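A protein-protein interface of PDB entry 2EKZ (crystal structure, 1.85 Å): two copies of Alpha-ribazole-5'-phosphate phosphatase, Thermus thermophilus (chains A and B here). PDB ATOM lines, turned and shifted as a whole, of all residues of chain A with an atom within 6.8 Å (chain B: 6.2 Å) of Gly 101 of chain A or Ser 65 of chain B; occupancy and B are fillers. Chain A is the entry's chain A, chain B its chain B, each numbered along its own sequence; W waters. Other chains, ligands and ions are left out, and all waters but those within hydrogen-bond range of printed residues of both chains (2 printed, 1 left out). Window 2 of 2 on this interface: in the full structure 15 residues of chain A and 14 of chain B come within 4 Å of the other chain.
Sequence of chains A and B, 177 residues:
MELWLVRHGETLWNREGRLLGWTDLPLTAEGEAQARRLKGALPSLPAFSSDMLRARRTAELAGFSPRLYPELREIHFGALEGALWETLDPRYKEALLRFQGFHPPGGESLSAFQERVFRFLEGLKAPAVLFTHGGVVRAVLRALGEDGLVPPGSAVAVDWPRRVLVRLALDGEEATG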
ATOM      1  N   ARG A  91      15.209  27.784  33.172  1.00  0.00           N
ATOM      2  CA  ARG A  91      16.324  27.334  32.347  1.00  0.00           C
ATOM      3  C   ARG A  91      16.110  27.759  30.899  1.00  0.00           C
ATOM      4  O   ARG A  91      17.033  28.257  30.253  1.00  0.00           O
ATOM      5  CB  ARG A  91      16.481  25.810  32.419  1.00  0.00           C
ATOM      6  CG  ARG A  91      15.298  25.019  31.878  1.00  0.00           C
ATOM      7  CD  ARG A  91      15.573  23.523  31.911  1.00  0.00           C
ATOM      8  NE  ARG A  91      14.399  22.742  31.529  1.00  0.00           N
ATOM      9  CZ  ARG A  91      14.356  21.414  31.519  1.00  0.00           C
ATOM     10  NH1 ARG A  91      15.425  20.712  31.869  1.00  0.00           N
ATOM     11  NH2 ARG A  91      13.244  20.786  31.162  1.00  0.00           N
ATOM     12  N   TYR A  92      14.895  27.555  30.394  1.00  0.00           N
ATOM     13  CA  TYR A  92      14.570  27.934  29.025  1.00  0.00           C
ATOM     14  C   TYR A  92      14.572  29.451  28.880  1.00  0.00           C
ATOM     15  O   TYR A  92      15.047  29.980  27.876  1.00  0.00           O
ATOM     16  CB  TYR A  92      13.205  27.372  28.617  1.00  0.00           C
ATOM     17  CG  TYR A  92      13.185  25.874  28.418  1.00  0.00           C
ATOM     18  CD1 TYR A  92      14.143  25.244  27.622  1.00  0.00           C
ATOM     19  CD2 TYR A  92      12.196  25.085  29.003  1.00  0.00           C
ATOM     20  CE1 TYR A  92      14.116  23.872  27.415  1.00  0.00           C
ATOM     21  CE2 TYR A  92      12.159  23.713  28.802  1.00  0.00           C
ATOM     22  CZ  TYR A  92      13.119  23.113  28.007  1.00  0.00           C
ATOM     23  OH  TYR A  92      13.085  21.758  27.804  1.00  0.00           O
ATOM     24  N   ALA A  95      18.164  30.542  28.751  1.00  0.00           N
ATOM     25  CA  ALA A  95      18.776  30.137  27.490  1.00  0.00           C
ATOM     26  C   ALA A  95      18.375  31.105  26.384  1.00  0.00           C
ATOM     27  O   ALA A  95      19.213  31.554  25.605  1.00  0.00           O
ATOM     28  CB  ALA A  95      18.351  28.718  27.128  1.00  0.00           C
ATOM     29  N   LEU A  96      17.088  31.427  26.318  1.00  0.00           N
ATOM     30  CA  LEU A  96      16.609  32.351  25.298  1.00  0.00           C
ATOM     31  C   LEU A  96      17.116  33.774  25.544  1.00  0.00           C
ATOM     32  O   LEU A  96      17.507  34.468  24.608  1.00  0.00           O
ATOM     33  CB  LEU A  96      15.076  32.317  25.243  1.00  0.00           C
ATOM     34  CG  LEU A  96      14.503  31.005  24.696  1.00  0.00           C
ATOM     35  CD1 LEU A  96      12.980  31.016  24.772  1.00  0.00           C
ATOM     36  CD2 LEU A  96      14.957  30.823  23.254  1.00  0.00           C
ATOM     37  N   ARG A  98      19.903  34.769  27.167  1.00  0.00           N
ATOM     38  CA  ARG A  98      21.335  34.849  26.900  1.00  0.00           C
ATOM     39  C   ARG A  98      21.646  34.347  25.493  1.00  0.00           C
ATOM     40  O   ARG A  98      22.785  34.434  25.026  1.00  0.00           O
ATOM     41  CB  ARG A  98      22.115  34.029  27.933  1.00  0.00           C
ATOM     42  CG  ARG A  98      21.825  34.414  29.378  1.00  0.00           C
ATOM     43  CD  ARG A  98      22.898  33.876  30.312  1.00  0.00           C
ATOM     44  NE  ARG A  98      24.191  34.507  30.059  1.00  0.00           N
ATOM     45  CZ  ARG A  98      25.336  34.127  30.617  1.00  0.00           C
ATOM     46  NH1 ARG A  98      25.359  33.109  31.467  1.00  0.00           N
ATOM     47  NH2 ARG A  98      26.460  34.765  30.324  1.00  0.00           N
ATOM     48  N   PHE A  99      20.621  33.824  24.826  1.00  0.00           N
ATOM     49  CA  PHE A  99      20.746  33.306  23.469  1.00  0.00           C
ATOM     50  C   PHE A  99      21.841  32.249  23.371  1.00  0.00           C
ATOM     51  O   PHE A  99      22.790  32.387  22.594  1.00  0.00           O
ATOM     52  CB  PHE A  99      21.040  34.450  22.494  1.00  0.00           C
ATOM     53  CG  PHE A  99      20.331  34.318  21.174  1.00  0.00           C
ATOM     54  CD1 PHE A  99      18.940  34.347  21.113  1.00  0.00           C
ATOM     55  CD2 PHE A  99      21.050  34.168  19.993  1.00  0.00           C
ATOM     56  CE1 PHE A  99      18.277  34.229  19.892  1.00  0.00           C
ATOM     57  CE2 PHE A  99      20.393  34.049  18.769  1.00  0.00           C
ATOM     58  CZ  PHE A  99      19.006  34.080  18.719  1.00  0.00           C
ATOM     59  N   GLN A 100      21.703  31.184  24.155  1.00  0.00           N
ATOM     60  CA  GLN A 100      22.690  30.111  24.141  1.00  0.00           C
ATOM     61  C   GLN A 100      22.209  28.878  24.892  1.00  0.00           C
ATOM     62  O   GLN A 100      21.449  28.984  25.856  1.00  0.00           O
ATOM     63  CB  GLN A 100      23.989  30.599  24.771  1.00  0.00           C
ATOM     64  CG  GLN A 100      23.836  30.979  26.225  1.00  0.00           C
ATOM     65  CD  GLN A 100      25.095  31.574  26.811  1.00  0.00           C
ATOM     66  OE1 GLN A 100      25.147  31.894  27.999  1.00  0.00           O
ATOM     67  NE2 GLN A 100      26.116  31.730  25.984  1.00  0.00           N
ATOM     68  N   GLY A 101      22.666  27.713  24.443  1.00  0.00           N
ATOM     69  CA  GLY A 101      22.302  26.460  25.081  1.00  0.00           C
ATOM     70  C   GLY A 101      20.808  26.225  25.196  1.00  0.00           C
ATOM     71  O   GLY A 101      20.302  25.909  26.276  1.00  0.00           O
ATOM     72  N   PHE A 102      20.102  26.383  24.082  1.00  0.00           N
ATOM     73  CA  PHE A 102      18.657  26.178  24.041  1.00  0.00           C
ATOM     74  C   PHE A 102      18.370  24.990  23.137  1.00  0.00           C
ATOM     75  O   PHE A 102      18.658  25.030  21.942  1.00  0.00           O
ATOM     76  CB  PHE A 102      17.962  27.423  23.484  1.00  0.00           C
ATOM     77  CG  PHE A 102      16.463  27.286  23.350  1.00  0.00           C
ATOM     78  CD1 PHE A 102      15.661  27.096  24.472  1.00  0.00           C
ATOM     79  CD2 PHE A 102      15.854  27.380  22.099  1.00  0.00           C
ATOM     80  CE1 PHE A 102      14.269  27.006  24.354  1.00  0.00           C
ATOM     81  CE2 PHE A 102      14.463  27.292  21.967  1.00  0.00           C
ATOM     82  CZ  PHE A 102      13.669  27.105  23.098  1.00  0.00           C
ATOM     83  N   HIS A 103      17.825  23.924  23.705  1.00  0.00           N
ATOM     84  CA  HIS A 103      17.506  22.750  22.911  1.00  0.00           C
ATOM     85  C   HIS A 103      16.173  22.193  23.380  1.00  0.00           C
ATOM     86  O   HIS A 103      16.116  21.298  24.225  1.00  0.00           O
ATOM     87  CB  HIS A 103      18.591  21.681  23.044  1.00  0.00           C
ATOM     88  CG  HIS A 103      18.727  20.813  21.830  1.00  0.00           C
ATOM     89  ND1 HIS A 103      17.649  20.449  21.051  1.00  0.00           N
ATOM     90  CD2 HIS A 103      19.813  20.236  21.263  1.00  0.00           C
ATOM     91  CE1 HIS A 103      18.065  19.686  20.057  1.00  0.00           C
ATOM     92  NE2 HIS A 103      19.374  19.541  20.163  1.00  0.00           N
ATOM     93  N   LEU A 110      19.419  26.199  19.397  1.00  0.00           N
ATOM     94  CA  LEU A 110      19.801  27.538  18.985  1.00  0.00           C
ATOM     95  C   LEU A 110      20.999  27.484  18.044  1.00  0.00           C
ATOM     96  O   LEU A 110      21.076  28.249  17.084  1.00  0.00           O
ATOM     97  CB  LEU A 110      20.144  28.399  20.195  1.00  0.00           C
ATOM     98  CG  LEU A 110      20.502  29.833  19.805  1.00  0.00           C
ATOM     99  CD1 LEU A 110      19.246  30.561  19.336  1.00  0.00           C
ATOM    100  CD2 LEU A 110      21.113  30.545  20.989  1.00  0.00           C
ATOM    101  N   SER A 111      21.933  26.578  18.322  1.00  0.00           N
ATOM    102  CA  SER A 111      23.121  26.428  17.487  1.00  0.00           C
ATOM    103  C   SER A 111      22.736  26.022  16.069  1.00  0.00           C
ATOM    104  O   SER A 111      23.300  26.521  15.095  1.00  0.00           O
ATOM    105  CB  SER A 111      24.062  25.374  18.085  1.00  0.00           C
ATOM    106  OG  SER A 111      24.539  25.794  19.351  1.00  0.00           O
ATOM    107  N   ALA B  47      29.308  31.240  20.052  1.00  0.00           N
ATOM    108  CA  ALA B  47      30.552  30.713  20.596  1.00  0.00           C
ATOM    109  C   ALA B  47      30.914  29.322  20.099  1.00  0.00           C
ATOM    110  O   ALA B  47      30.047  28.477  19.858  1.00  0.00           O
ATOM    111  CB  ALA B  47      30.493  30.715  22.127  1.00  0.00           C
ATOM    112  N   ALA B  59      34.980  28.412  28.599  1.00  0.00           N
ATOM    113  CA  ALA B  59      33.778  28.927  27.949  1.00  0.00           C
ATOM    114  C   ALA B  59      32.596  28.965  28.919  1.00  0.00           C
ATOM    115  O   ALA B  59      31.870  29.960  28.996  1.00  0.00           O
ATOM    116  CB  ALA B  59      33.433  28.072  26.735  1.00  0.00           C
ATOM    117  N   GLU B  60      32.407  27.878  29.657  1.00  0.00           N
ATOM    118  CA  GLU B  60      31.313  27.787  30.620  1.00  0.00           C
ATOM    119  C   GLU B  60      31.392  28.881  31.683  1.00  0.00           C
ATOM    120  O   GLU B  60      30.410  29.579  31.940  1.00  0.00           O
ATOM    121  CB  GLU B  60      31.322  26.408  31.289  1.00  0.00           C
ATOM    122  CG  GLU B  60      30.323  26.255  32.422  1.00  0.00           C
ATOM    123  CD  GLU B  60      30.451  24.920  33.133  1.00  0.00           C
ATOM    124  OE1 GLU B  60      31.598  24.475  33.359  1.00  0.00           O
ATOM    125  OE2 GLU B  60      29.410  24.324  33.479  1.00  0.00           O
ATOM    126  N   GLY B  63      30.517  32.315  30.710  1.00  0.00           N
ATOM    127  CA  GLY B  63      29.107  32.501  30.400  1.00  0.00           C
ATOM    128  C   GLY B  63      28.626  32.080  29.022  1.00  0.00           C
ATOM    129  O   GLY B  63      27.612  32.590  28.538  1.00  0.00           O
ATOM    130  N   PHE B  64      29.331  31.142  28.395  1.00  0.00           N
ATOM    131  CA  PHE B  64      28.970  30.672  27.060  1.00  0.00           C
ATOM    132  C   PHE B  64      28.654  29.173  26.999  1.00  0.00           C
ATOM    133  O   PHE B  64      29.065  28.406  27.868  1.00  0.00           O
ATOM    134  CB  PHE B  64      30.120  30.962  26.086  1.00  0.00           C
ATOM    135  CG  PHE B  64      30.387  32.427  25.871  1.00  0.00           C
ATOM    136  CD1 PHE B  64      31.195  33.139  26.752  1.00  0.00           C
ATOM    137  CD2 PHE B  64      29.844  33.089  24.773  1.00  0.00           C
ATOM    138  CE1 PHE B  64      31.460  34.497  26.539  1.00  0.00           C
ATOM    139  CE2 PHE B  64      30.103  34.444  24.550  1.00  0.00           C
ATOM    140  CZ  PHE B  64      30.914  35.148  25.434  1.00  0.00           C
ATOM    141  N   SER B  65      27.923  28.781  25.956  1.00  0.00           N
ATOM    142  CA  SER B  65      27.553  27.384  25.687  1.00  0.00           C
ATOM    143  C   SER B  65      27.990  27.202  24.237  1.00  0.00           C
ATOM    144  O   SER B  65      27.188  27.317  23.313  1.00  0.00           O
ATOM    145  CB  SER B  65      26.039  27.189  25.801  1.00  0.00           C
ATOM    146  OG  SER B  65      25.580  27.552  27.085  1.00  0.00           O
ATOM    147  N   PRO B  66      29.277  26.904  24.023  1.00  0.00           N
ATOM    148  CA  PRO B  66      29.869  26.720  22.698  1.00  0.00           C
ATOM    149  C   PRO B  66      29.623  25.435  21.935  1.00  0.00           C
ATOM    150  O   PRO B  66      29.360  24.382  22.517  1.00  0.00           O
ATOM    151  CB  PRO B  66      31.354  26.907  22.976  1.00  0.00           C
ATOM    152  CG  PRO B  66      31.498  26.182  24.289  1.00  0.00           C
ATOM    153  CD  PRO B  66      30.293  26.693  25.075  1.00  0.00           C
ATOM    154  N   ARG B  67      29.716  25.548  20.616  1.00  0.00           N
ATOM    155  CA  ARG B  67      29.607  24.405  19.726  1.00  0.00           C
ATOM    156  C   ARG B  67      31.043  23.904  19.763  1.00  0.00           C
ATOM    157  O   ARG B  67      31.981  24.704  19.668  1.00  0.00           O
ATOM    158  CB  ARG B  67      29.232  24.857  18.316  1.00  0.00           C
ATOM    159  CG  ARG B  67      27.799  25.352  18.213  1.00  0.00           C
ATOM    160  CD  ARG B  67      27.551  26.111  16.924  1.00  0.00           C
ATOM    161  NE  ARG B  67      27.834  25.317  15.735  1.00  0.00           N
ATOM    162  CZ  ARG B  67      27.649  25.757  14.495  1.00  0.00           C
ATOM    163  NH1 ARG B  67      27.176  26.981  14.289  1.00  0.00           N
ATOM    164  NH2 ARG B  67      27.945  24.981  13.461  1.00  0.00           N
HETATM  165  O   HOH W   1      27.211  30.932  23.989  1.00  0.00           O
HETATM  166  O   HOH W   2      24.471  27.893  22.419  1.00  0.00           O
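Gln 100 of chain A touches Phe 64 of chain B (NE2 to CA, 3.2 Å).
Gly 101 of chain A touches Ser 65 of chain B.
CG of Arg 67 of chain B touches OG of Ser 111 of chain A (3.5 Å).
Water W1 bridges NE2 of Gln 100 of chain A and N of Ser 65 of chain B.
Water W2 lies within hydrogen-bond range of N of Gly 101 of chain A (2.7 Å) and O of Ser 65 of chain B (2.9 Å).
No position is printed for both chains.
Of the 6 pairs that touch across the chains among the printed residues, none has its exchanged pair printed and touching as well.
N of Ser 65 of chain B lies close to NE2 of Gln 100 of chain A, at 3.5 Å.
The side-chain amide oxygen (OE1) of Gln 100 of chain A sits close to the backbone carbonyl oxygen (O) of Gly 63 of chain B.
O of Gly 63 of chain B lies within hydrogen-bond range of NH2 of Arg 98 of chain A, 3.0 Å away.
Of the 12 printed residues of chain A, 4 touch a printed residue of chain B.
Printed residues of chain A that touch a printed residue of chain B: Arg 98, Gln 100, Gly 101 and Ser 111.
Along chain A the printed residues that touch a printed residue of chain B span positions 98 to 111.
Of the 8 printed residues of chain B, 4 touch a printed residue of chain A.
Among the printed residues, 6 pairs touch across the chains.
O of Ala 47 of chain B is in hydrogen-bond range of N of Arg 67 of chain B, at 3.0 Å.
The backbone carbonyl oxygen (O) of Ala 59 of chain B is in hydrogen-bond range of the backbone NH (N) of Phe 64 of chain B, at 2.9 Å.
The side-chain amide oxygen of Gln 100 of chain A lies close to the guanidinium group of Arg 98 of chain A (3.5 Å).
The backbone NH (N) of Gln 100 of chain A is in hydrogen-bond range of the backbone carbonyl oxygen (O) of Ala 95 of chain A.
Gly 101 of chain A touches just one residue of chain B: Ser 65 (3.7 Å).
Of the printed residues of chain A, Gly 63 of chain B touches Arg 98 (3.0 Å) and Gln 100 (2.6 Å).
Of the printed residues of chain A, Arg 67 of chain B touches Ser 111.
Printed residues of chain B within 4 Å of Arg 98 of chain A: Gly 63.
The nearest printed residue of chain B that does not touch Gly 101 of chain A is Phe 64 of chain B (6.7 Å).
The nearest residue of chain A that does not touch Ser 65 of chain B is Ser 111 of chain A (5.0 Å).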
